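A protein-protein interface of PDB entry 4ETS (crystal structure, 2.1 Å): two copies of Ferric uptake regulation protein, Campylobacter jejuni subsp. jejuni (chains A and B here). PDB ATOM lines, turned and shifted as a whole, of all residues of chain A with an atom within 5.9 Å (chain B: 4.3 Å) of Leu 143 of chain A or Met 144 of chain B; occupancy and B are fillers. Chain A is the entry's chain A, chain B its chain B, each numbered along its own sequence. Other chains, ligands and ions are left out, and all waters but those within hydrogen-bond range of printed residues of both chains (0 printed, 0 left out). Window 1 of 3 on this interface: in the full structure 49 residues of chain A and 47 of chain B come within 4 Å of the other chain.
The backbone NH of Val 11 of chain A sits at hydrogen-bond distance from the side-chain amide oxygen of Gln 145 of chain B, 3.2 Å away.
N of Glu 12 of chain A is in hydrogen-bond range of OH of Tyr 147 of chain B, 3.3 Å away.
N of Tyr 147 of chain B lies within hydrogen-bond range of O of Gly 141 of chain A.
N of Leu 143 of chain A sits at hydrogen-bond distance from O of Gln 145 of chain B (2.9 Å).
The backbone carbonyl oxygen (O) of Gln 145 of chain A is in hydrogen-bond range of the backbone NH (N) of Leu 143 of chain B, at 2.8 Å.
O of His 142 of chain A is in hydrogen-bond range of NE2 of His 104 of chain A.
O of Met 144 of chain B lies within hydrogen-bond range of N of His 107 of chain B (3.5 Å).
The backbone carbonyl oxygen (O) of His 107 of chain B is in hydrogen-bond range of the backbone NH (N) of Leu 146 of chain B (2.8 Å).
OH of Tyr 147 of chain B is in hydrogen-bond range of OE1 of Gln 145 of chain B, at 2.6 Å.
Tyr 147 of chain B touches Val 11 of chain A.
Met 144 of chain B touches Gln 128 of chain A.
Leu 146 of chain B touches Gly 141 of chain A (CA to O, 3.8 Å).
O of Gln 145 of chain B touches CA of His 142 of chain A, 3.2 Å away.
Tyr 147 of chain B touches His 142 of chain A (CD2 to N, 3.3 Å).
Leu 143 of chain B touches Leu 143 of chain A.
CA of Met 144 of chain B touches O of Leu 143 of chain A, at 3.2 Å.
Tyr 147 of chain B touches Leu 143 of chain A.
O of Leu 143 of chain B touches CA of Met 144 of chain A, at 3.3 Å.
Printed residues of chain B within 4 Å of Leu 143 of chain A: Leu 143 (3.5 Å), Met 144 (3.2 Å), Gln 145 (2.9 Å) and Tyr 147 (3.8 Å).
Printed residues of chain A within 4 Å of Met 144 of chain B: Gln 128 and Leu 143.
Of the printed residues of chain B, Glu 12 of chain A touches Tyr 147 (3.3 Å).
Of the printed residues of chain A, Leu 146 of chain B touches Gly 141 (3.8 Å).
Printed residues of chain A within 4 Å of Gln 145 of chain B: Val 11, His 142 and Leu 143.
Printed residues of chain B within 4 Å of Met 144 of chain A: Leu 143 (3.3 Å).
Of the printed residues of chain A, Tyr 147 of chain B touches Val 11, Glu 12, Gly 141, His 142 and Leu 143.
Phe 119 of chain B touches none of the printed residues of chain A.
Ile 124 of chain A touches none of the printed residues of chain B.
The nearest printed residue of chain B that does not touch Leu 143 of chain A is Leu 146 of chain B (5.1 Å).
Hydrophobic or aromatic side chains of chain A within 4 Å of the printed part of chain B: Val 11, His 142 and Leu 143.
Along chain A the printed residues that touch a printed residue of chain B span positions 11 to 145.
Printed residues of chain B that touch a printed residue of chain A: Leu 143, Met 144, Gln 145, Leu 146 and Tyr 147.
Among the printed residues, no Asp or Glu carboxylate lies within 4 Å of a Lys or Arg side-chain nitrogen of the other chain.
Leu 143 of chain A touches its own counterpart, Leu 143 of chain B.
Leu 143 of chain A touches Met 144 of chain B, and with the chains exchanged Met 144 of chain A touches Leu 143 of chain B.
Leu 143 of chain A touches Gln 145 of chain B, and with the chains exchanged Gln 145 of chain A touches Leu 143 of chain B.
Positions printed for both chains: 106, 124, 143, 144 and 145.
Of the 14 pairs that touch across the chains among the printed residues, 5 have their exchanged pair printed and touching as well.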
ATOM      1  N   VAL A  11      12.991  10.675 -31.550  1.00  0.00           N
ATOM      2  CA  VAL A  11      12.026  10.541 -30.459  1.00  0.00           C
ATOM      3  C   VAL A  11      12.506  11.357 -29.235  1.00  0.00           C
ATOM      4  O   VAL A  11      11.702  11.814 -28.441  1.00  0.00           O
ATOM      5  CB  VAL A  11      11.871   9.079 -30.037  1.00  0.00           C
ATOM      6  CG1 VAL A  11      11.162   8.998 -28.685  1.00  0.00           C
ATOM      7  CG2 VAL A  11      11.071   8.323 -31.107  1.00  0.00           C
ATOM      8  N   GLU A  12      13.828  11.432 -29.061  1.00  0.00           N
ATOM      9  CA  GLU A  12      14.434  12.186 -27.945  1.00  0.00           C
ATOM     10  C   GLU A  12      13.911  13.678 -27.967  1.00  0.00           C
ATOM     11  O   GLU A  12      13.432  14.213 -26.986  1.00  0.00           O
ATOM     12  CB  GLU A  12      15.943  12.170 -28.133  1.00  0.00           C
ATOM     13  CG  GLU A  12      16.701  13.068 -27.221  1.00  0.00           C
ATOM     14  CD  GLU A  12      18.158  12.780 -27.245  1.00  0.00           C
ATOM     15  OE1 GLU A  12      18.932  13.228 -28.129  1.00  0.00           O
ATOM     16  OE2 GLU A  12      18.553  12.076 -26.348  1.00  0.00           O
ATOM     17  N   HIS A 104      19.251   7.139 -18.021  1.00  0.00           N
ATOM     18  CA  HIS A 104      17.966   6.556 -17.771  1.00  0.00           C
ATOM     19  C   HIS A 104      18.068   5.062 -18.177  1.00  0.00           C
ATOM     20  O   HIS A 104      19.092   4.649 -18.727  1.00  0.00           O
ATOM     21  CB  HIS A 104      16.903   7.268 -18.586  1.00  0.00           C
ATOM     22  CG  HIS A 104      17.115   7.121 -20.071  1.00  0.00           C
ATOM     23  ND1 HIS A 104      17.592   8.148 -20.876  1.00  0.00           N
ATOM     24  CD2 HIS A 104      16.994   6.033 -20.877  1.00  0.00           C
ATOM     25  CE1 HIS A 104      17.720   7.696 -22.119  1.00  0.00           C
ATOM     26  NE2 HIS A 104      17.356   6.418 -22.147  1.00  0.00           N
ATOM     27  N   ASP A 106      15.801   1.424 -19.728  1.00  0.00           N
ATOM     28  CA  ASP A 106      15.099   1.020 -20.928  1.00  0.00           C
ATOM     29  C   ASP A 106      13.831   0.304 -20.496  1.00  0.00           C
ATOM     30  O   ASP A 106      13.666  -0.006 -19.296  1.00  0.00           O
ATOM     31  CB  ASP A 106      16.022   0.060 -21.704  1.00  0.00           C
ATOM     32  CG  ASP A 106      17.371   0.662 -21.967  1.00  0.00           C
ATOM     33  OD1 ASP A 106      17.441   1.835 -22.437  1.00  0.00           O
ATOM     34  OD2 ASP A 106      18.375  -0.016 -21.597  1.00  0.00           O
ATOM     35  N   ILE A 124      24.410  -4.537 -23.592  1.00  0.00           N
ATOM     36  CA  ILE A 124      23.792  -3.691 -24.633  1.00  0.00           C
ATOM     37  C   ILE A 124      24.402  -2.276 -24.568  1.00  0.00           C
ATOM     38  O   ILE A 124      24.753  -1.744 -25.605  1.00  0.00           O
ATOM     39  CB  ILE A 124      22.261  -3.606 -24.508  1.00  0.00           C
ATOM     40  CG1 ILE A 124      21.677  -5.013 -24.899  1.00  0.00           C
ATOM     41  CG2 ILE A 124      21.717  -2.374 -25.441  1.00  0.00           C
ATOM     42  CD1 ILE A 124      20.189  -5.185 -24.666  1.00  0.00           C
ATOM     43  N   GLN A 128      26.450  -0.350 -27.652  1.00  0.00           N
ATOM     44  CA  GLN A 128      25.978   0.977 -28.154  1.00  0.00           C
ATOM     45  C   GLN A 128      27.169   1.947 -28.221  1.00  0.00           C
ATOM     46  O   GLN A 128      27.359   2.620 -29.214  1.00  0.00           O
ATOM     47  CB  GLN A 128      24.899   1.565 -27.216  1.00  0.00           C
ATOM     48  CG  GLN A 128      23.485   0.909 -27.403  1.00  0.00           C
ATOM     49  CD  GLN A 128      22.597   1.331 -26.338  1.00  0.00           C
ATOM     50  OE1 GLN A 128      23.011   2.093 -25.449  1.00  0.00           O
ATOM     51  NE2 GLN A 128      21.376   0.872 -26.380  1.00  0.00           N
ATOM     52  N   GLY A 141      22.991  10.208 -26.324  1.00  0.00           N
ATOM     53  CA  GLY A 141      21.626   9.856 -25.843  1.00  0.00           C
ATOM     54  C   GLY A 141      21.210   8.509 -26.496  1.00  0.00           C
ATOM     55  O   GLY A 141      21.898   8.073 -27.432  1.00  0.00           O
ATOM     56  N   HIS A 142      20.085   7.908 -26.045  1.00  0.00           N
ATOM     57  CA  HIS A 142      19.520   6.766 -26.736  1.00  0.00           C
ATOM     58  C   HIS A 142      18.159   6.469 -26.212  1.00  0.00           C
ATOM     59  O   HIS A 142      17.763   6.948 -25.124  1.00  0.00           O
ATOM     60  CB  HIS A 142      20.406   5.509 -26.643  1.00  0.00           C
ATOM     61  CG  HIS A 142      20.390   4.837 -25.302  1.00  0.00           C
ATOM     62  ND1 HIS A 142      21.143   5.297 -24.226  1.00  0.00           N
ATOM     63  CD2 HIS A 142      19.725   3.729 -24.859  1.00  0.00           C
ATOM     64  CE1 HIS A 142      20.970   4.478 -23.190  1.00  0.00           C
ATOM     65  NE2 HIS A 142      20.094   3.542 -23.544  1.00  0.00           N
ATOM     66  N   LEU A 143      17.453   5.654 -26.985  1.00  0.00           N
ATOM     67  CA  LEU A 143      16.204   5.153 -26.571  1.00  0.00           C
ATOM     68  C   LEU A 143      16.047   3.675 -26.989  1.00  0.00           C
ATOM     69  O   LEU A 143      16.345   3.277 -28.172  1.00  0.00           O
ATOM     70  CB  LEU A 143      15.159   5.977 -27.269  1.00  0.00           C
ATOM     71  CG  LEU A 143      13.794   5.330 -27.205  1.00  0.00           C
ATOM     72  CD1 LEU A 143      13.129   5.534 -25.815  1.00  0.00           C
ATOM     73  CD2 LEU A 143      13.017   5.858 -28.334  1.00  0.00           C
ATOM     74  N   MET A 144      15.597   2.864 -26.036  1.00  0.00           N
ATOM     75  CA  MET A 144      15.347   1.481 -26.305  1.00  0.00           C
ATOM     76  C   MET A 144      14.080   1.027 -25.695  1.00  0.00           C
ATOM     77  O   MET A 144      13.936   1.048 -24.463  1.00  0.00           O
ATOM     78  CB  MET A 144      16.525   0.613 -25.797  1.00  0.00           C
ATOM     79  CG  MET A 144      16.266  -0.898 -25.987  1.00  0.00           C
ATOM     80  SD  MET A 144      17.582  -1.818 -25.124  1.00  0.00           S
ATOM     81  CE  MET A 144      17.773  -3.017 -26.334  1.00  0.00           C
ATOM     82  N   GLN A 145      13.178   0.557 -26.532  1.00  0.00           N
ATOM     83  CA  GLN A 145      11.977  -0.152 -26.057  1.00  0.00           C
ATOM     84  C   GLN A 145      11.853  -1.520 -26.715  1.00  0.00           C
ATOM     85  O   GLN A 145      12.115  -1.641 -27.904  1.00  0.00           O
ATOM     86  CB  GLN A 145      10.698   0.643 -26.357  1.00  0.00           C
ATOM     87  CG  GLN A 145      10.754   2.135 -25.898  1.00  0.00           C
ATOM     88  CD  GLN A 145       9.337   2.767 -25.857  1.00  0.00           C
ATOM     89  OE1 GLN A 145       8.479   2.544 -26.756  1.00  0.00           O
ATOM     90  NE2 GLN A 145       9.088   3.544 -24.820  1.00  0.00           N
ATOM     91  N   ASP B 106      18.290  -0.656 -36.778  1.00  0.00           N
ATOM     92  CA  ASP B 106      18.405   0.419 -35.785  1.00  0.00           C
ATOM     93  C   ASP B 106      19.175   1.560 -36.369  1.00  0.00           C
ATOM     94  O   ASP B 106      19.769   1.387 -37.444  1.00  0.00           O
ATOM     95  CB  ASP B 106      19.095  -0.130 -34.504  1.00  0.00           C
ATOM     96  CG  ASP B 106      18.482  -1.487 -34.083  1.00  0.00           C
ATOM     97  OD1 ASP B 106      17.236  -1.546 -33.988  1.00  0.00           O
ATOM     98  OD2 ASP B 106      19.235  -2.482 -33.868  1.00  0.00           O
ATOM     99  N   HIS B 107      19.114   2.734 -35.713  1.00  0.00           N
ATOM    100  CA  HIS B 107      19.633   3.948 -36.281  1.00  0.00           C
ATOM    101  C   HIS B 107      20.338   4.805 -35.268  1.00  0.00           C
ATOM    102  O   HIS B 107      19.892   4.988 -34.081  1.00  0.00           O
ATOM    103  CB  HIS B 107      18.493   4.745 -36.950  1.00  0.00           C
ATOM    104  CG  HIS B 107      17.766   3.947 -37.987  1.00  0.00           C
ATOM    105  ND1 HIS B 107      16.690   3.146 -37.684  1.00  0.00           N
ATOM    106  CD2 HIS B 107      18.008   3.761 -39.320  1.00  0.00           C
ATOM    107  CE1 HIS B 107      16.275   2.522 -38.780  1.00  0.00           C
ATOM    108  NE2 HIS B 107      17.027   2.917 -39.795  1.00  0.00           N
ATOM    109  N   PHE B 119      22.149   0.386 -38.529  1.00  0.00           N
ATOM    110  CA  PHE B 119      23.000  -0.671 -38.031  1.00  0.00           C
ATOM    111  C   PHE B 119      22.130  -1.787 -37.433  1.00  0.00           C
ATOM    112  O   PHE B 119      20.952  -1.590 -37.096  1.00  0.00           O
ATOM    113  CB  PHE B 119      24.009  -0.117 -36.975  1.00  0.00           C
ATOM    114  CG  PHE B 119      23.339   0.241 -35.584  1.00  0.00           C
ATOM    115  CD1 PHE B 119      22.870   1.550 -35.322  1.00  0.00           C
ATOM    116  CD2 PHE B 119      23.167  -0.738 -34.590  1.00  0.00           C
ATOM    117  CE1 PHE B 119      22.261   1.879 -34.073  1.00  0.00           C
ATOM    118  CE2 PHE B 119      22.607  -0.414 -33.312  1.00  0.00           C
ATOM    119  CZ  PHE B 119      22.148   0.919 -33.071  1.00  0.00           C
ATOM    120  N   ILE B 124      23.553  -7.379 -29.525  1.00  0.00           N
ATOM    121  CA  ILE B 124      22.426  -6.638 -28.929  1.00  0.00           C
ATOM    122  C   ILE B 124      21.112  -7.399 -29.225  1.00  0.00           C
ATOM    123  O   ILE B 124      20.245  -7.505 -28.354  1.00  0.00           O
ATOM    124  CB  ILE B 124      22.300  -5.197 -29.571  1.00  0.00           C
ATOM    125  CG1 ILE B 124      23.391  -4.314 -29.033  1.00  0.00           C
ATOM    126  CG2 ILE B 124      20.896  -4.622 -29.247  1.00  0.00           C
ATOM    127  CD1 ILE B 124      23.416  -2.910 -29.647  1.00  0.00           C
ATOM    128  N   LEU B 143      12.377  -0.907 -30.614  1.00  0.00           N
ATOM    129  CA  LEU B 143      12.845   0.320 -31.205  1.00  0.00           C
ATOM    130  C   LEU B 143      14.169   0.674 -30.521  1.00  0.00           C
ATOM    131  O   LEU B 143      14.273   0.635 -29.278  1.00  0.00           O
ATOM    132  CB  LEU B 143      11.778   1.418 -31.022  1.00  0.00           C
ATOM    133  CG  LEU B 143      12.245   2.842 -31.452  1.00  0.00           C
ATOM    134  CD1 LEU B 143      12.300   2.955 -33.017  1.00  0.00           C
ATOM    135  CD2 LEU B 143      11.342   3.918 -30.878  1.00  0.00           C
ATOM    136  N   MET B 144      15.193   1.004 -31.315  1.00  0.00           N
ATOM    137  CA  MET B 144      16.442   1.454 -30.749  1.00  0.00           C
ATOM    138  C   MET B 144      16.978   2.575 -31.615  1.00  0.00           C
ATOM    139  O   MET B 144      17.246   2.362 -32.804  1.00  0.00           O
ATOM    140  CB  MET B 144      17.459   0.305 -30.664  1.00  0.00           C
ATOM    141  CG  MET B 144      18.771   0.626 -29.934  1.00  0.00           C
ATOM    142  SD  MET B 144      19.974  -0.735 -30.102  1.00  0.00           S
ATOM    143  CE  MET B 144      21.503   0.099 -29.797  1.00  0.00           C
ATOM    144  N   GLN B 145      17.102   3.768 -31.026  1.00  0.00           N
ATOM    145  CA  GLN B 145      17.752   4.941 -31.678  1.00  0.00           C
ATOM    146  C   GLN B 145      18.897   5.371 -30.812  1.00  0.00           C
ATOM    147  O   GLN B 145      18.727   5.439 -29.590  1.00  0.00           O
ATOM    148  CB  GLN B 145      16.795   6.113 -31.715  1.00  0.00           C
ATOM    149  CG  GLN B 145      15.564   5.777 -32.425  1.00  0.00           C
ATOM    150  CD  GLN B 145      14.870   7.053 -32.890  1.00  0.00           C
ATOM    151  OE1 GLN B 145      14.808   8.085 -32.148  1.00  0.00           O
ATOM    152  NE2 GLN B 145      14.308   6.992 -34.086  1.00  0.00           N
ATOM    153  N   LEU B 146      20.051   5.656 -31.393  1.00  0.00           N
ATOM    154  CA  LEU B 146      21.181   6.280 -30.678  1.00  0.00           C
ATOM    155  C   LEU B 146      21.256   7.743 -31.188  1.00  0.00           C
ATOM    156  O   LEU B 146      21.059   8.015 -32.427  1.00  0.00           O
ATOM    157  CB  LEU B 146      22.469   5.611 -31.083  1.00  0.00           C
ATOM    158  CG  LEU B 146      22.787   4.209 -30.510  1.00  0.00           C
ATOM    159  CD1 LEU B 146      21.679   3.538 -29.900  1.00  0.00           C
ATOM    160  CD2 LEU B 146      23.803   3.262 -31.214  1.00  0.00           C
ATOM    161  N   TYR B 147      21.607   8.648 -30.305  1.00  0.00           N
ATOM    162  CA  TYR B 147      21.682  10.072 -30.651  1.00  0.00           C
ATOM    163  C   TYR B 147      23.076  10.484 -30.280  1.00  0.00           C
ATOM    164  O   TYR B 147      23.613   9.975 -29.305  1.00  0.00           O
ATOM    165  CB  TYR B 147      20.770  10.874 -29.754  1.00  0.00           C
ATOM    166  CG  TYR B 147      19.417  10.316 -29.769  1.00  0.00           C
ATOM    167  CD1 TYR B 147      18.640  10.413 -30.920  1.00  0.00           C
ATOM    168  CD2 TYR B 147      18.895   9.683 -28.622  1.00  0.00           C
ATOM    169  CE1 TYR B 147      17.374   9.864 -30.949  1.00  0.00           C
ATOM    170  CE2 TYR B 147      17.613   9.168 -28.645  1.00  0.00           C
ATOM    171  CZ  TYR B 147      16.895   9.227 -29.806  1.00  0.00           C
ATOM    172  OH  TYR B 147      15.621   8.734 -29.803  1.00  0.00           O
